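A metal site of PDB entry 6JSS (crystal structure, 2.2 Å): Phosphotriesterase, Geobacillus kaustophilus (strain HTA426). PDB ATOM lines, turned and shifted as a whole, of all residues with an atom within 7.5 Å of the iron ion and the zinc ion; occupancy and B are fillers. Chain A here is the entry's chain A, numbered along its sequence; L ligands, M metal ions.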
ATOM      1  N   HIS A  27     -31.590  24.754  16.499  1.00  0.00           N
ATOM      2  CA  HIS A  27     -30.870  25.348  17.667  1.00  0.00           C
ATOM      3  C   HIS A  27     -29.350  25.241  17.549  1.00  0.00           C
ATOM      4  O   HIS A  27     -28.823  24.231  17.890  1.00  0.00           O
ATOM      5  CB  HIS A  27     -31.362  24.699  18.967  1.00  0.00           C
ATOM      6  CG  HIS A  27     -30.963  25.378  20.229  1.00  0.00           C
ATOM      7  ND1 HIS A  27     -31.857  25.710  21.160  1.00  0.00           N
ATOM      8  CD2 HIS A  27     -29.776  25.757  20.704  1.00  0.00           C
ATOM      9  CE1 HIS A  27     -31.271  26.268  22.166  1.00  0.00           C
ATOM     10  NE2 HIS A  27     -29.996  26.303  21.932  1.00  0.00           N
ATOM     11  N   GLU A  28     -28.707  26.303  17.046  1.00  0.00           N
ATOM     12  CA  GLU A  28     -27.233  26.330  16.878  1.00  0.00           C
ATOM     13  C   GLU A  28     -26.723  27.741  17.207  1.00  0.00           C
ATOM     14  O   GLU A  28     -27.416  28.713  16.853  1.00  0.00           O
ATOM     15  CB  GLU A  28     -26.848  25.918  15.462  1.00  0.00           C
ATOM     16  CG  GLU A  28     -27.379  24.558  15.054  1.00  0.00           C
ATOM     17  CD  GLU A  28     -26.739  23.387  15.789  1.00  0.00           C
ATOM     18  OE1 GLU A  28     -25.644  23.574  16.351  1.00  0.00           O
ATOM     19  OE2 GLU A  28     -27.341  22.292  15.785  1.00  0.00           O
ATOM     20  N   HIS A  29     -25.552  27.833  17.848  1.00  0.00           N
ATOM     21  CA  HIS A  29     -24.976  29.135  18.223  1.00  0.00           C
ATOM     22  C   HIS A  29     -23.705  29.447  17.428  1.00  0.00           C
ATOM     23  O   HIS A  29     -22.726  28.821  17.656  1.00  0.00           O
ATOM     24  CB  HIS A  29     -24.702  29.188  19.712  1.00  0.00           C
ATOM     25  CG  HIS A  29     -25.909  29.058  20.564  1.00  0.00           C
ATOM     26  ND1 HIS A  29     -26.678  30.101  20.908  1.00  0.00           N
ATOM     27  CD2 HIS A  29     -26.440  28.001  21.163  1.00  0.00           C
ATOM     28  CE1 HIS A  29     -27.642  29.693  21.668  1.00  0.00           C
ATOM     29  NE2 HIS A  29     -27.517  28.432  21.829  1.00  0.00           N
ATOM     30  N   PHE A  32     -21.368  32.527  21.180  1.00  0.00           N
ATOM     31  CA  PHE A  32     -22.006  32.429  22.481  1.00  0.00           C
ATOM     32  C   PHE A  32     -20.982  32.750  23.563  1.00  0.00           C
ATOM     33  O   PHE A  32     -19.830  32.337  23.471  1.00  0.00           O
ATOM     34  CB  PHE A  32     -22.609  31.048  22.736  1.00  0.00           C
ATOM     35  CG  PHE A  32     -23.149  30.885  24.134  1.00  0.00           C
ATOM     36  CD1 PHE A  32     -24.460  31.255  24.443  1.00  0.00           C
ATOM     37  CD2 PHE A  32     -22.337  30.408  25.152  1.00  0.00           C
ATOM     38  CE1 PHE A  32     -24.945  31.118  25.745  1.00  0.00           C
ATOM     39  CE2 PHE A  32     -22.823  30.272  26.454  1.00  0.00           C
ATOM     40  CZ  PHE A  32     -24.124  30.619  26.742  1.00  0.00           C
ATOM     41  N   ASP A  72     -30.710  30.456  15.460  1.00  0.00           N
ATOM     42  CA  ASP A  72     -29.684  30.766  16.438  1.00  0.00           C
ATOM     43  C   ASP A  72     -30.351  31.477  17.599  1.00  0.00           C
ATOM     44  O   ASP A  72     -30.619  32.691  17.525  1.00  0.00           O
ATOM     45  CB  ASP A  72     -28.584  31.646  15.814  1.00  0.00           C
ATOM     46  CG  ASP A  72     -27.405  31.864  16.748  1.00  0.00           C
ATOM     47  OD1 ASP A  72     -27.622  31.970  17.964  1.00  0.00           O
ATOM     48  OD2 ASP A  72     -26.252  31.930  16.251  1.00  0.00           O
ATOM     49  N   PRO A  73     -30.639  30.788  18.677  1.00  0.00           N
ATOM     50  CA  PRO A  73     -31.402  31.407  19.760  1.00  0.00           C
ATOM     51  C   PRO A  73     -30.508  31.957  20.862  1.00  0.00           C
ATOM     52  O   PRO A  73     -30.835  31.815  22.048  1.00  0.00           O
ATOM     53  CB  PRO A  73     -32.270  30.255  20.264  1.00  0.00           C
ATOM     54  CG  PRO A  73     -31.363  29.063  20.082  1.00  0.00           C
ATOM     55  CD  PRO A  73     -30.442  29.356  18.890  1.00  0.00           C
ATOM     56  N   THR A  74     -29.377  32.557  20.497  1.00  0.00           N
ATOM     57  CA  THR A  74     -28.476  33.109  21.496  1.00  0.00           C
ATOM     58  C   THR A  74     -29.164  34.220  22.289  1.00  0.00           C
ATOM     59  O   THR A  74     -29.639  35.188  21.680  1.00  0.00           O
ATOM     60  CB  THR A  74     -27.226  33.663  20.821  1.00  0.00           C
ATOM     61  OG1 THR A  74     -26.511  32.590  20.215  1.00  0.00           O
ATOM     62  CG2 THR A  74     -26.340  34.355  21.848  1.00  0.00           C
ATOM     63  N   PRO A  75     -29.256  34.120  23.614  1.00  0.00           N
ATOM     64  CA  PRO A  75     -29.904  35.170  24.398  1.00  0.00           C
ATOM     65  C   PRO A  75     -29.233  36.524  24.229  1.00  0.00           C
ATOM     66  O   PRO A  75     -28.067  36.628  23.824  1.00  0.00           O
ATOM     67  CB  PRO A  75     -29.773  34.677  25.848  1.00  0.00           C
ATOM     68  CG  PRO A  75     -29.645  33.164  25.704  1.00  0.00           C
ATOM     69  CD  PRO A  75     -28.860  32.962  24.449  1.00  0.00           C
ATOM     70  N   TYR A 104     -31.785  31.524  31.668  1.00  0.00           N
ATOM     71  CA  TYR A 104     -32.352  31.186  32.983  1.00  0.00           C
ATOM     72  C   TYR A 104     -31.444  31.702  34.094  1.00  0.00           C
ATOM     73  O   TYR A 104     -30.277  32.041  33.876  1.00  0.00           O
ATOM     74  CB  TYR A 104     -32.595  29.675  33.128  1.00  0.00           C
ATOM     75  CG  TYR A 104     -31.343  28.821  33.271  1.00  0.00           C
ATOM     76  CD1 TYR A 104     -30.562  28.456  32.171  1.00  0.00           C
ATOM     77  CD2 TYR A 104     -30.938  28.355  34.516  1.00  0.00           C
ATOM     78  CE1 TYR A 104     -29.423  27.674  32.314  1.00  0.00           C
ATOM     79  CE2 TYR A 104     -29.824  27.578  34.672  1.00  0.00           C
ATOM     80  CZ  TYR A 104     -29.061  27.245  33.587  1.00  0.00           C
ATOM     81  OH  TYR A 104     -27.944  26.468  33.798  1.00  0.00           O
ATOM     82  N   GLU A 107     -27.574  30.501  34.874  1.00  0.00           N
ATOM     83  CA  GLU A 107     -26.526  30.688  33.870  1.00  0.00           C
ATOM     84  C   GLU A 107     -26.731  32.012  33.145  1.00  0.00           C
ATOM     85  O   GLU A 107     -26.497  32.135  31.940  1.00  0.00           O
ATOM     86  CB  GLU A 107     -26.464  29.506  32.903  1.00  0.00           C
ATOM     87  CG  GLU A 107     -25.296  28.546  33.195  1.00  0.00           C
ATOM     88  CD  GLU A 107     -25.396  27.209  32.466  1.00  0.00           C
ATOM     89  OE1 GLU A 107     -24.726  26.248  32.900  1.00  0.00           O
ATOM     90  OE2 GLU A 107     -26.137  27.124  31.457  1.00  0.00           O
ATOM     91  N   KCX A 149     -36.887  33.528  22.778  1.00  0.00           N
ATOM     92  CA  KCX A 149     -36.159  32.497  23.506  1.00  0.00           C
ATOM     93  CB  KCX A 149     -34.642  32.670  23.318  1.00  0.00           C
ATOM     94  CG  KCX A 149     -33.775  31.696  24.143  1.00  0.00           C
ATOM     95  CD  KCX A 149     -34.146  30.258  23.801  1.00  0.00           C
ATOM     96  CE  KCX A 149     -33.227  29.269  24.510  1.00  0.00           C
ATOM     97  NZ  KCX A 149     -31.804  29.413  24.011  1.00  0.00           N
ATOM     98  C   KCX A 149     -36.515  32.571  24.988  1.00  0.00           C
ATOM     99  O   KCX A 149     -36.461  33.640  25.598  1.00  0.00           O
ATOM    100  CX  KCX A 149     -30.929  28.450  24.276  1.00  0.00           C
ATOM    101  OQ1 KCX A 149     -31.313  27.452  24.923  1.00  0.00           O
ATOM    102  OQ2 KCX A 149     -29.755  28.543  23.876  1.00  0.00           O
ATOM    103  N   LEU A 150     -36.915  31.434  25.544  1.00  0.00           N
ATOM    104  CA  LEU A 150     -37.248  31.311  26.972  1.00  0.00           C
ATOM    105  C   LEU A 150     -36.388  30.273  27.661  1.00  0.00           C
ATOM    106  O   LEU A 150     -36.007  29.278  27.043  1.00  0.00           O
ATOM    107  CB  LEU A 150     -38.710  30.921  27.130  1.00  0.00           C
ATOM    108  CG  LEU A 150     -39.724  32.004  26.843  1.00  0.00           C
ATOM    109  CD1 LEU A 150     -41.108  31.442  27.117  1.00  0.00           C
ATOM    110  CD2 LEU A 150     -39.405  33.220  27.693  1.00  0.00           C
ATOM    111  N   ALA A 151     -36.118  30.430  28.952  1.00  0.00           N
ATOM    112  CA  ALA A 151     -35.321  29.430  29.645  1.00  0.00           C
ATOM    113  C   ALA A 151     -35.792  29.243  31.096  1.00  0.00           C
ATOM    114  O   ALA A 151     -36.188  30.200  31.747  1.00  0.00           O
ATOM    115  CB  ALA A 151     -33.846  29.822  29.626  1.00  0.00           C
ATOM    116  N   THR A 181     -37.633  27.219  23.631  1.00  0.00           N
ATOM    117  CA  THR A 181     -37.269  27.222  25.046  1.00  0.00           C
ATOM    118  C   THR A 181     -36.028  26.384  25.322  1.00  0.00           C
ATOM    119  O   THR A 181     -35.633  25.531  24.528  1.00  0.00           O
ATOM    120  CB  THR A 181     -38.408  26.731  25.954  1.00  0.00           C
ATOM    121  OG1 THR A 181     -38.340  25.308  26.047  1.00  0.00           O
ATOM    122  CG2 THR A 181     -39.755  27.138  25.438  1.00  0.00           C
ATOM    123  N   HIS A 182     -35.445  26.653  26.487  1.00  0.00           N
ATOM    124  CA  HIS A 182     -34.351  25.904  27.083  1.00  0.00           C
ATOM    125  C   HIS A 182     -34.881  25.225  28.348  1.00  0.00           C
ATOM    126  O   HIS A 182     -35.505  25.882  29.177  1.00  0.00           O
ATOM    127  CB  HIS A 182     -33.199  26.866  27.416  1.00  0.00           C
ATOM    128  CG  HIS A 182     -32.185  26.344  28.378  1.00  0.00           C
ATOM    129  ND1 HIS A 182     -30.840  26.240  28.047  1.00  0.00           N
ATOM    130  CD2 HIS A 182     -32.283  25.956  29.674  1.00  0.00           C
ATOM    131  CE1 HIS A 182     -30.169  25.781  29.098  1.00  0.00           C
ATOM    132  NE2 HIS A 182     -31.026  25.604  30.098  1.00  0.00           N
ATOM    133  N   THR A 183     -34.662  23.907  28.477  1.00  0.00           N
ATOM    134  CA  THR A 183     -34.922  23.218  29.743  1.00  0.00           C
ATOM    135  C   THR A 183     -33.602  22.805  30.371  1.00  0.00           C
ATOM    136  O   THR A 183     -32.670  22.406  29.676  1.00  0.00           O
ATOM    137  CB  THR A 183     -35.850  21.985  29.618  1.00  0.00           C
ATOM    138  OG1 THR A 183     -35.308  21.014  28.698  1.00  0.00           O
ATOM    139  CG2 THR A 183     -37.240  22.395  29.177  1.00  0.00           C
ATOM    140  N   GLN A 184     -33.515  22.932  31.691  1.00  0.00           N
ATOM    141  CA  GLN A 184     -32.269  22.669  32.385  1.00  0.00           C
ATOM    142  C   GLN A 184     -32.292  21.246  32.944  1.00  0.00           C
ATOM    143  O   GLN A 184     -33.190  20.908  33.712  1.00  0.00           O
ATOM    144  CB  GLN A 184     -32.058  23.714  33.490  1.00  0.00           C
ATOM    145  CG  GLN A 184     -30.702  23.667  34.174  1.00  0.00           C
ATOM    146  CD  GLN A 184     -29.512  23.761  33.219  1.00  0.00           C
ATOM    147  OE1 GLN A 184     -29.625  24.229  32.080  1.00  0.00           O
ATOM    148  NE2 GLN A 184     -28.366  23.300  33.690  1.00  0.00           N
ATOM    149  N   GLY A 209     -37.345  22.988  24.374  1.00  0.00           N
ATOM    150  CA  GLY A 209     -35.976  22.594  24.079  1.00  0.00           C
ATOM    151  C   GLY A 209     -35.318  21.769  25.153  1.00  0.00           C
ATOM    152  O   GLY A 209     -35.859  21.614  26.218  1.00  0.00           O
ATOM    153  N   HIS A 210     -34.200  21.187  24.748  1.00  0.00           N
ATOM    154  CA  HIS A 210     -33.285  20.344  25.536  1.00  0.00           C
ATOM    155  C   HIS A 210     -34.071  19.150  26.094  1.00  0.00           C
ATOM    156  O   HIS A 210     -33.814  18.767  27.200  1.00  0.00           O
ATOM    157  CB  HIS A 210     -32.496  21.203  26.543  1.00  0.00           C
ATOM    158  CG  HIS A 210     -31.811  22.432  26.026  1.00  0.00           C
ATOM    159  ND1 HIS A 210     -31.214  22.500  24.816  1.00  0.00           N
ATOM    160  CD2 HIS A 210     -31.608  23.644  26.591  1.00  0.00           C
ATOM    161  CE1 HIS A 210     -30.686  23.685  24.649  1.00  0.00           C
ATOM    162  NE2 HIS A 210     -30.906  24.402  25.726  1.00  0.00           N
ATOM    163  N   ASP A 233     -32.025  18.572  20.864  1.00  0.00           N
ATOM    164  CA  ASP A 233     -31.195  19.607  20.250  1.00  0.00           C
ATOM    165  C   ASP A 233     -29.793  19.675  20.850  1.00  0.00           C
ATOM    166  O   ASP A 233     -29.077  20.634  20.571  1.00  0.00           O
ATOM    167  CB  ASP A 233     -31.895  20.960  20.365  1.00  0.00           C
ATOM    168  CG  ASP A 233     -32.333  21.252  21.788  1.00  0.00           C
ATOM    169  OD1 ASP A 233     -31.766  20.637  22.704  1.00  0.00           O
ATOM    170  OD2 ASP A 233     -33.249  22.076  22.002  1.00  0.00           O
ATOM    171  N   ARG A 234     -29.366  18.685  21.631  1.00  0.00           N
ATOM    172  CA  ARG A 234     -28.019  18.705  22.188  1.00  0.00           C
ATOM    173  C   ARG A 234     -27.236  17.436  21.865  1.00  0.00           C
ATOM    174  O   ARG A 234     -26.420  16.969  22.660  1.00  0.00           O
ATOM    175  CB  ARG A 234     -28.055  18.938  23.688  1.00  0.00           C
ATOM    176  CG  ARG A 234     -28.348  20.390  24.025  1.00  0.00           C
ATOM    177  CD  ARG A 234     -28.262  20.645  25.520  1.00  0.00           C
ATOM    178  NE  ARG A 234     -27.876  22.028  25.785  1.00  0.00           N
ATOM    179  CZ  ARG A 234     -27.754  22.526  26.995  1.00  0.00           C
ATOM    180  NH1 ARG A 234     -27.993  21.754  28.044  1.00  0.00           N
ATOM    181  NH2 ARG A 234     -27.410  23.806  27.167  1.00  0.00           N
ATOM    182  N   HIS A 269     -27.846  20.306  17.580  1.00  0.00           N
ATOM    183  CA  HIS A 269     -26.690  20.077  18.434  1.00  0.00           C
ATOM    184  C   HIS A 269     -26.475  21.124  19.515  1.00  0.00           C
ATOM    185  O   HIS A 269     -25.772  20.820  20.487  1.00  0.00           O
ATOM    186  CB  HIS A 269     -25.387  20.043  17.647  1.00  0.00           C
ATOM    187  CG  HIS A 269     -25.444  19.310  16.355  1.00  0.00           C
ATOM    188  ND1 HIS A 269     -25.819  19.907  15.182  1.00  0.00           N
ATOM    189  CD2 HIS A 269     -25.122  18.024  16.043  1.00  0.00           C
ATOM    190  CE1 HIS A 269     -25.738  19.030  14.198  1.00  0.00           C
ATOM    191  NE2 HIS A 269     -25.314  17.875  14.697  1.00  0.00           N
ATOM    192  N   ASP A 270     -26.995  22.344  19.365  1.00  0.00           N
ATOM    193  CA  ASP A 270     -26.721  23.404  20.333  1.00  0.00           C
ATOM    194  C   ASP A 270     -25.218  23.703  20.359  1.00  0.00           C
ATOM    195  O   ASP A 270     -24.611  23.845  21.430  1.00  0.00           O
ATOM    196  CB  ASP A 270     -27.254  23.007  21.709  1.00  0.00           C
ATOM    197  CG  ASP A 270     -27.421  24.163  22.682  1.00  0.00           C
ATOM    198  OD1 ASP A 270     -27.428  25.355  22.286  1.00  0.00           O
ATOM    199  OD2 ASP A 270     -27.590  23.855  23.883  1.00  0.00           O
ATOM    200  N   THR A 271     -24.594  23.767  19.191  1.00  0.00           N
ATOM    201  CA  THR A 271     -23.157  24.015  19.169  1.00  0.00           C
ATOM    202  C   THR A 271     -22.869  25.456  19.536  1.00  0.00           C
ATOM    203  O   THR A 271     -23.715  26.339  19.397  1.00  0.00           O
ATOM    204  CB  THR A 271     -22.549  23.727  17.783  1.00  0.00           C
ATOM    205  OG1 THR A 271     -23.217  24.488  16.778  1.00  0.00           O
ATOM    206  CG2 THR A 271     -22.660  22.250  17.463  1.00  0.00           C
ATOM    207  N   VAL A 272     -21.665  25.685  20.059  1.00  0.00           N
ATOM    208  CA  VAL A 272     -21.088  27.011  20.149  1.00  0.00           C
ATOM    209  C   VAL A 272     -19.882  27.025  19.226  1.00  0.00           C
ATOM    210  O   VAL A 272     -18.859  26.390  19.499  1.00  0.00           O
ATOM    211  CB  VAL A 272     -20.671  27.389  21.570  1.00  0.00           C
ATOM    212  CG1 VAL A 272     -20.051  28.811  21.562  1.00  0.00           C
ATOM    213  CG2 VAL A 272     -21.881  27.289  22.486  1.00  0.00           C
HETATM  214  O1  LIG L   1     -28.139  26.335  25.227  1.00  0.00           O
HETATM  215 FE    FE M   1     -28.498  26.995  23.212  1.00  0.00          FE
HETATM  216 ZN    ZN M   2     -30.098  26.208  26.046  1.00  0.00          ZN
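The side-chain hydroxyl (OG1) of Thr 183 lies within hydrogen-bond range of the backbone carbonyl oxygen (O) of His 210 (3.1 Å).
ND1 of His 210 sits at hydrogen-bond distance from OD1 of Asp 233 (2.9 Å).
The backbone carbonyl oxygen (O) of Pro 73 is in hydrogen-bond range of NZ of KCX 149 (3.2 Å).
NE2 of His 182 sits at hydrogen-bond distance from OE1 of Gln 184, at 2.8 Å.
The backbone carbonyl oxygen of Leu 150 sits at hydrogen-bond distance from the backbone NH of His 182 (2.7 Å).
The guanidinium group (NE) of Arg 234 is in salt-bridge range of the side-chain carboxylate (OD2) of Asp 270, 2.7 Å away.
The backbone NH of Asp 270 lies within hydrogen-bond range of the backbone carbonyl oxygen of Asp 233, 3.0 Å away.
The backbone carbonyl oxygen (O) of Thr 271 is in hydrogen-bond range of the backbone NH (N) of His 29.
Within 4 Å of the iron ion: His 27, His 29, KCX 149 and Asp 270.
The nearest printed residue that does not touch the iron ion is His 210 (4.2 Å).
Arg 234 touches the zinc ion.
Four residues have an atom within 4 Å of the zinc ion: KCX 149, His 182, His 210 and Arg 234.
The nearest printed residue that does not touch the zinc ion is His 27 (4.1 Å).
The iron ion is bound by a ring nitrogen (NE2) of His 27 (2.1 Å), OQ2 of KCX 149 (2.1 Å), an oxygen (O1) of the ligand (2.2 Å), the side-chain carboxylate of Asp 270 (2.2 Å) and a ring nitrogen (NE2) of His 29 (2.2 Å).
The zinc ion is bound by a ring nitrogen (NE2) of His 210.
The zinc ion is bound by OQ1 of KCX 149.
An oxygen (O1) of the ligand binds the zinc ion.
ND1 of His 182 is bound to the zinc ion, 2.1 Å away.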
